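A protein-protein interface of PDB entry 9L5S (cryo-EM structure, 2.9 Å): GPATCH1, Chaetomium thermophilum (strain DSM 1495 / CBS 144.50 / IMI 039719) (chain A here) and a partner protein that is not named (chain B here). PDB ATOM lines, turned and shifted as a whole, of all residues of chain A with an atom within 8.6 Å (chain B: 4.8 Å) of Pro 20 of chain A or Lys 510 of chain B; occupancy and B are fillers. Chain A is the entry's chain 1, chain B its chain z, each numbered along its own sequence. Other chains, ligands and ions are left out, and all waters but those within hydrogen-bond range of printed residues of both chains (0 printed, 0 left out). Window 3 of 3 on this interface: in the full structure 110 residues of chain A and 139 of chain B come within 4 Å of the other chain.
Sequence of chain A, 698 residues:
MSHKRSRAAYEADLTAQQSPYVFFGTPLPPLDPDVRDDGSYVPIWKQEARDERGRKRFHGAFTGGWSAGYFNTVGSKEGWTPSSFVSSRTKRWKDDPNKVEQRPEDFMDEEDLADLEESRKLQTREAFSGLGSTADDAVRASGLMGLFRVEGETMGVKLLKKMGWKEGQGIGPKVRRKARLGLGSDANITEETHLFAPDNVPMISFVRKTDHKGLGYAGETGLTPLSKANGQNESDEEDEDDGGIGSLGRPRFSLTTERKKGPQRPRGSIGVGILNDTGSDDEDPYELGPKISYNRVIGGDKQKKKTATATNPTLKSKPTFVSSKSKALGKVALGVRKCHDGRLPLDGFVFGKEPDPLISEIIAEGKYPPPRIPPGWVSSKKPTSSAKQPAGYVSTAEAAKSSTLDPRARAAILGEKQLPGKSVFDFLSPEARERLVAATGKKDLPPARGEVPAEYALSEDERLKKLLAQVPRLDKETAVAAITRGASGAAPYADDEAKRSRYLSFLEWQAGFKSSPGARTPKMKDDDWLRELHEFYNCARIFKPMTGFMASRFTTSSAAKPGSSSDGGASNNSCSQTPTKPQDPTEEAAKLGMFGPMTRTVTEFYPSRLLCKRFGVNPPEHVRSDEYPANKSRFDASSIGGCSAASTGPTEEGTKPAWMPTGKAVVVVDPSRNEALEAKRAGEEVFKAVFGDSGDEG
Hydrophobic or aromatic side chains of chain A that line the printed part of chain B: Pro 20, Tyr 21, Val 22 and Leu 28.
Of the 7 printed residues of chain B, 4 touch a printed residue of chain A.
Hydrophobic or aromatic side chains of chain B within 4 Å of the printed part of chain A: Phe 511 and Ala 512.
The backbone carbonyl oxygen (O) of Leu 28 of chain A is in hydrogen-bond range of the guanidinium group (NH2) of Arg 509 of chain B, at 2.9 Å.
Ala 16 of chain A touches none of the printed residues of chain B.
Gln 17 of chain A touches none of the printed residues of chain B.
Of the printed residues of chain B, Pro 20 of chain A touches Lys 510.
Of the printed residues of chain B, Pro 27 of chain A touches Ala 512 (3.8 Å).
Printed residues of chain A within 4 Å of Arg 509 of chain B: Gln 18, Ser 19 and Leu 28.
Printed residues of chain A within 4 Å of Lys 510 of chain B: Gln 18 (3.4 Å), Ser 19 (3.96 Å), Pro 20 (3.7 Å) and Tyr 21 (3.8 Å).
Printed residues of chain A within 4 Å of Ala 512 of chain B: Val 22 (3.3 Å), Pro 27 (3.8 Å) and Leu 28 (3.7 Å).
The nearest residue of chain A that does not touch Lys 510 of chain B is Val 22 of chain A (4.3 Å).
Arg 509 of chain B touches Gln 18 of chain A.
Gln 18 of chain A touches Lys 510 of chain B.
O of Arg 509 of chain B touches CB of Ser 19 of chain A, 3.4 Å away.
Lys 510 of chain B touches Ser 19 of chain A (O to CA, 3.96 Å).
Lys 510 of chain B touches Pro 20 of chain A (CE to CD, 3.7 Å).
Tyr 21 of chain A touches Lys 510 of chain B (O to O, 3.8 Å).
Tyr 21 of chain A touches Phe 511 of chain B.
Ala 512 of chain B touches Val 22 of chain A.
O of Ala 512 of chain B touches CA of Pro 27 of chain A (3.8 Å).
Ala 512 of chain B touches Leu 28 of chain A (CB to CG, 3.7 Å).
O of Thr 15 of chain A sits at hydrogen-bond distance from OG of Ser 19 of chain A (2.8 Å).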
ATOM      1  N   ASP A  13      12.880  11.378  17.210  1.00  0.00           N
ATOM      2  CA  ASP A  13      13.637  12.618  17.092  1.00  0.00           C
ATOM      3  C   ASP A  13      14.697  12.552  15.997  1.00  0.00           C
ATOM      4  O   ASP A  13      15.123  13.603  15.513  1.00  0.00           O
ATOM      5  CB  ASP A  13      14.243  13.046  18.445  1.00  0.00           C
ATOM      6  CG  ASP A  13      15.303  12.092  18.983  1.00  0.00           C
ATOM      7  OD1 ASP A  13      15.549  11.023  18.404  1.00  0.00           O
ATOM      8  OD2 ASP A  13      15.906  12.431  20.023  1.00  0.00           O
ATOM      9  N   LEU A  14      15.080  11.352  15.543  1.00  0.00           N
ATOM     10  CA  LEU A  14      15.916  11.254  14.352  1.00  0.00           C
ATOM     11  C   LEU A  14      15.146  11.666  13.102  1.00  0.00           C
ATOM     12  O   LEU A  14      15.693  12.347  12.226  1.00  0.00           O
ATOM     13  CB  LEU A  14      16.453   9.830  14.216  1.00  0.00           C
ATOM     14  CG  LEU A  14      17.564   9.571  13.200  1.00  0.00           C
ATOM     15  CD1 LEU A  14      18.688  10.582  13.357  1.00  0.00           C
ATOM     16  CD2 LEU A  14      18.086   8.157  13.374  1.00  0.00           C
ATOM     17  N   THR A  15      13.873  11.264  13.003  1.00  0.00           N
ATOM     18  CA  THR A  15      13.025  11.725  11.909  1.00  0.00           C
ATOM     19  C   THR A  15      12.758  13.222  12.017  1.00  0.00           C
ATOM     20  O   THR A  15      12.674  13.919  10.999  1.00  0.00           O
ATOM     21  CB  THR A  15      11.710  10.943  11.902  1.00  0.00           C
ATOM     22  OG1 THR A  15      11.983   9.544  12.048  1.00  0.00           O
ATOM     23  CG2 THR A  15      10.956  11.165  10.596  1.00  0.00           C
ATOM     24  N   ALA A  16      12.614  13.727  13.246  1.00  0.00           N
ATOM     25  CA  ALA A  16      12.433  15.163  13.446  1.00  0.00           C
ATOM     26  C   ALA A  16      13.672  15.947  13.020  1.00  0.00           C
ATOM     27  O   ALA A  16      13.557  17.038  12.448  1.00  0.00           O
ATOM     28  CB  ALA A  16      12.094  15.450  14.907  1.00  0.00           C
ATOM     29  N   GLN A  17      14.863  15.416  13.302  1.00  0.00           N
ATOM     30  CA  GLN A  17      16.093  16.106  12.924  1.00  0.00           C
ATOM     31  C   GLN A  17      16.338  16.031  11.420  1.00  0.00           C
ATOM     32  O   GLN A  17      16.708  17.034  10.797  1.00  0.00           O
ATOM     33  CB  GLN A  17      17.277  15.520  13.694  1.00  0.00           C
ATOM     34  CG  GLN A  17      18.598  16.244  13.471  1.00  0.00           C
ATOM     35  CD  GLN A  17      19.474  15.564  12.436  1.00  0.00           C
ATOM     36  OE1 GLN A  17      19.399  14.350  12.244  1.00  0.00           O
ATOM     37  NE2 GLN A  17      20.308  16.345  11.760  1.00  0.00           N
ATOM     38  N   GLN A  18      16.147  14.852  10.820  1.00  0.00           N
ATOM     39  CA  GLN A  18      16.447  14.690   9.400  1.00  0.00           C
ATOM     40  C   GLN A  18      15.418  15.394   8.523  1.00  0.00           C
ATOM     41  O   GLN A  18      15.776  16.009   7.511  1.00  0.00           O
ATOM     42  CB  GLN A  18      16.529  13.206   9.043  1.00  0.00           C
ATOM     43  CG  GLN A  18      17.854  12.555   9.410  1.00  0.00           C
ATOM     44  CD  GLN A  18      18.153  11.330   8.571  1.00  0.00           C
ATOM     45  OE1 GLN A  18      17.372  10.956   7.695  1.00  0.00           O
ATOM     46  NE2 GLN A  18      19.290  10.696   8.834  1.00  0.00           N
ATOM     47  N   SER A  19      14.140  15.318   8.889  1.00  0.00           N
ATOM     48  CA  SER A  19      13.054  15.927   8.121  1.00  0.00           C
ATOM     49  C   SER A  19      12.228  16.806   9.050  1.00  0.00           C
ATOM     50  O   SER A  19      11.150  16.405   9.511  1.00  0.00           O
ATOM     51  CB  SER A  19      12.187  14.863   7.449  1.00  0.00           C
ATOM     52  OG  SER A  19      11.680  13.943   8.401  1.00  0.00           O
ATOM     53  N   PRO A  20      12.704  18.020   9.349  1.00  0.00           N
ATOM     54  CA  PRO A  20      11.955  18.892  10.268  1.00  0.00           C
ATOM     55  C   PRO A  20      10.742  19.553   9.644  1.00  0.00           C
ATOM     56  O   PRO A  20       9.722  19.701  10.332  1.00  0.00           O
ATOM     57  CB  PRO A  20      12.998  19.946  10.687  1.00  0.00           C
ATOM     58  CG  PRO A  20      14.318  19.481  10.102  1.00  0.00           C
ATOM     59  CD  PRO A  20      13.965  18.644   8.921  1.00  0.00           C
ATOM     60  N   TYR A  21      10.811  19.956   8.375  1.00  0.00           N
ATOM     61  CA  TYR A  21       9.717  20.665   7.723  1.00  0.00           C
ATOM     62  C   TYR A  21       8.816  19.730   6.922  1.00  0.00           C
ATOM     63  O   TYR A  21       8.780  19.795   5.692  1.00  0.00           O
ATOM     64  CB  TYR A  21      10.253  21.776   6.823  1.00  0.00           C
ATOM     65  CG  TYR A  21       9.309  22.951   6.714  1.00  0.00           C
ATOM     66  CD1 TYR A  21       9.412  24.030   7.581  1.00  0.00           C
ATOM     67  CD2 TYR A  21       8.301  22.969   5.757  1.00  0.00           C
ATOM     68  CE1 TYR A  21       8.546  25.103   7.490  1.00  0.00           C
ATOM     69  CE2 TYR A  21       7.428  24.038   5.661  1.00  0.00           C
ATOM     70  CZ  TYR A  21       7.555  25.100   6.531  1.00  0.00           C
ATOM     71  OH  TYR A  21       6.692  26.168   6.438  1.00  0.00           O
ATOM     72  N   VAL A  22       8.089  18.849   7.608  1.00  0.00           N
ATOM     73  CA  VAL A  22       7.062  18.026   6.967  1.00  0.00           C
ATOM     74  C   VAL A  22       5.745  18.386   7.647  1.00  0.00           C
ATOM     75  O   VAL A  22       5.352  17.796   8.654  1.00  0.00           O
ATOM     76  CB  VAL A  22       7.375  16.535   7.057  1.00  0.00           C
ATOM     77  CG1 VAL A  22       6.370  15.738   6.239  1.00  0.00           C
ATOM     78  CG2 VAL A  22       8.793  16.253   6.578  1.00  0.00           C
ATOM     79  N   PHE A  23       5.053  19.378   7.086  1.00  0.00           N
ATOM     80  CA  PHE A  23       3.730  19.747   7.568  1.00  0.00           C
ATOM     81  C   PHE A  23       2.613  19.201   6.692  1.00  0.00           C
ATOM     82  O   PHE A  23       1.438  19.451   6.984  1.00  0.00           O
ATOM     83  CB  PHE A  23       3.614  21.270   7.675  1.00  0.00           C
ATOM     84  CG  PHE A  23       4.496  21.868   8.732  1.00  0.00           C
ATOM     85  CD1 PHE A  23       4.111  21.850  10.063  1.00  0.00           C
ATOM     86  CD2 PHE A  23       5.714  22.438   8.398  1.00  0.00           C
ATOM     87  CE1 PHE A  23       4.920  22.396  11.043  1.00  0.00           C
ATOM     88  CE2 PHE A  23       6.528  22.986   9.375  1.00  0.00           C
ATOM     89  CZ  PHE A  23       6.130  22.965  10.697  1.00  0.00           C
ATOM     90  N   PHE A  24       2.950  18.468   5.635  1.00  0.00           N
ATOM     91  CA  PHE A  24       1.963  17.842   4.767  1.00  0.00           C
ATOM     92  C   PHE A  24       2.424  16.426   4.464  1.00  0.00           C
ATOM     93  O   PHE A  24       3.590  16.212   4.121  1.00  0.00           O
ATOM     94  CB  PHE A  24       1.780  18.638   3.469  1.00  0.00           C
ATOM     95  CG  PHE A  24       1.171  19.997   3.673  1.00  0.00           C
ATOM     96  CD1 PHE A  24      -0.203  20.163   3.676  1.00  0.00           C
ATOM     97  CD2 PHE A  24       1.976  21.111   3.861  1.00  0.00           C
ATOM     98  CE1 PHE A  24      -0.765  21.414   3.865  1.00  0.00           C
ATOM     99  CE2 PHE A  24       1.421  22.363   4.050  1.00  0.00           C
ATOM    100  CZ  PHE A  24       0.048  22.515   4.052  1.00  0.00           C
ATOM    101  N   PRO A  27       6.441  12.095   6.897  1.00  0.00           N
ATOM    102  CA  PRO A  27       7.890  12.110   6.670  1.00  0.00           C
ATOM    103  C   PRO A  27       8.451  10.709   6.485  1.00  0.00           C
ATOM    104  O   PRO A  27       7.925   9.725   7.010  1.00  0.00           O
ATOM    105  CB  PRO A  27       8.444  12.763   7.943  1.00  0.00           C
ATOM    106  CG  PRO A  27       7.385  12.550   8.973  1.00  0.00           C
ATOM    107  CD  PRO A  27       6.080  12.585   8.238  1.00  0.00           C
ATOM    108  N   LEU A  28       9.537  10.632   5.720  1.00  0.00           N
ATOM    109  CA  LEU A  28      10.174   9.354   5.453  1.00  0.00           C
ATOM    110  C   LEU A  28      10.976   8.890   6.670  1.00  0.00           C
ATOM    111  O   LEU A  28      11.446   9.712   7.462  1.00  0.00           O
ATOM    112  CB  LEU A  28      11.092   9.463   4.236  1.00  0.00           C
ATOM    113  CG  LEU A  28      10.462   9.945   2.927  1.00  0.00           C
ATOM    114  CD1 LEU A  28      11.438   9.772   1.772  1.00  0.00           C
ATOM    115  CD2 LEU A  28       9.156   9.218   2.638  1.00  0.00           C
ATOM    116  N   SER B 506      19.205  13.909   0.605  1.00  0.00           N
ATOM    117  CA  SER B 506      18.917  14.385   1.956  1.00  0.00           C
ATOM    118  C   SER B 506      18.152  15.705   1.937  1.00  0.00           C
ATOM    119  O   SER B 506      17.201  15.885   2.707  1.00  0.00           O
ATOM    120  CB  SER B 506      20.214  14.532   2.748  1.00  0.00           C
ATOM    121  OG  SER B 506      20.989  15.612   2.260  1.00  0.00           O
ATOM    122  N   VAL B 507      18.551  16.641   1.072  1.00  0.00           N
ATOM    123  CA  VAL B 507      17.813  17.897   0.975  1.00  0.00           C
ATOM    124  C   VAL B 507      16.477  17.713   0.269  1.00  0.00           C
ATOM    125  O   VAL B 507      15.565  18.525   0.464  1.00  0.00           O
ATOM    126  CB  VAL B 507      18.643  18.997   0.287  1.00  0.00           C
ATOM    127  CG1 VAL B 507      19.956  19.215   1.028  1.00  0.00           C
ATOM    128  CG2 VAL B 507      18.893  18.674  -1.177  1.00  0.00           C
ATOM    129  N   LYS B 508      16.329  16.665  -0.549  1.00  0.00           N
ATOM    130  CA  LYS B 508      15.002  16.295  -1.024  1.00  0.00           C
ATOM    131  C   LYS B 508      14.202  15.607   0.072  1.00  0.00           C
ATOM    132  O   LYS B 508      12.967  15.662   0.069  1.00  0.00           O
ATOM    133  CB  LYS B 508      15.111  15.395  -2.255  1.00  0.00           C
ATOM    134  CG  LYS B 508      15.179  16.156  -3.570  1.00  0.00           C
ATOM    135  CD  LYS B 508      15.753  15.294  -4.683  1.00  0.00           C
ATOM    136  CE  LYS B 508      15.190  15.695  -6.037  1.00  0.00           C
ATOM    137  NZ  LYS B 508      13.728  15.428  -6.134  1.00  0.00           N
ATOM    138  N   ARG B 509      14.886  14.956   1.014  1.00  0.00           N
ATOM    139  CA  ARG B 509      14.239  14.351   2.170  1.00  0.00           C
ATOM    140  C   ARG B 509      13.998  15.340   3.302  1.00  0.00           C
ATOM    141  O   ARG B 509      13.334  14.982   4.281  1.00  0.00           O
ATOM    142  CB  ARG B 509      15.070  13.178   2.690  1.00  0.00           C
ATOM    143  CG  ARG B 509      14.849  11.881   1.935  1.00  0.00           C
ATOM    144  CD  ARG B 509      14.971  10.707   2.877  1.00  0.00           C
ATOM    145  NE  ARG B 509      14.410  11.026   4.184  1.00  0.00           N
ATOM    146  CZ  ARG B 509      14.497  10.239   5.246  1.00  0.00           C
ATOM    147  NH1 ARG B 509      15.120   9.074   5.191  1.00  0.00           N
ATOM    148  NH2 ARG B 509      13.944  10.629   6.391  1.00  0.00           N
ATOM    149  N   LYS B 510      14.527  16.561   3.198  1.00  0.00           N
ATOM    150  CA  LYS B 510      14.253  17.578   4.207  1.00  0.00           C
ATOM    151  C   LYS B 510      12.797  18.022   4.171  1.00  0.00           C
ATOM    152  O   LYS B 510      12.259  18.472   5.189  1.00  0.00           O
ATOM    153  CB  LYS B 510      15.177  18.780   4.005  1.00  0.00           C
ATOM    154  CG  LYS B 510      15.419  19.605   5.258  1.00  0.00           C
ATOM    155  CD  LYS B 510      16.531  19.011   6.104  1.00  0.00           C
ATOM    156  CE  LYS B 510      16.973  19.976   7.192  1.00  0.00           C
ATOM    157  NZ  LYS B 510      17.551  21.225   6.624  1.00  0.00           N
ATOM    158  N   PHE B 511      12.147  17.903   3.011  1.00  0.00           N
ATOM    159  CA  PHE B 511      10.756  18.306   2.844  1.00  0.00           C
ATOM    160  C   PHE B 511       9.906  17.152   2.325  1.00  0.00           C
ATOM    161  O   PHE B 511       8.850  17.385   1.727  1.00  0.00           O
ATOM    162  CB  PHE B 511      10.663  19.501   1.895  1.00  0.00           C
ATOM    163  CG  PHE B 511      11.517  20.665   2.306  1.00  0.00           C
ATOM    164  CD1 PHE B 511      11.085  21.555   3.274  1.00  0.00           C
ATOM    165  CD2 PHE B 511      12.760  20.865   1.723  1.00  0.00           C
ATOM    166  CE1 PHE B 511      11.877  22.623   3.655  1.00  0.00           C
ATOM    167  CE2 PHE B 511      13.555  21.931   2.097  1.00  0.00           C
ATOM    168  CZ  PHE B 511      13.112  22.812   3.063  1.00  0.00           C
ATOM    169  N   ALA B 512      10.348  15.916   2.542  1.00  0.00           N
ATOM    170  CA  ALA B 512       9.734  14.762   1.901  1.00  0.00           C
ATOM    171  C   ALA B 512       8.383  14.427   2.517  1.00  0.00           C
ATOM    172  O   ALA B 512       8.183  14.540   3.729  1.00  0.00           O
ATOM    173  CB  ALA B 512      10.658  13.551   2.004  1.00  0.00           C
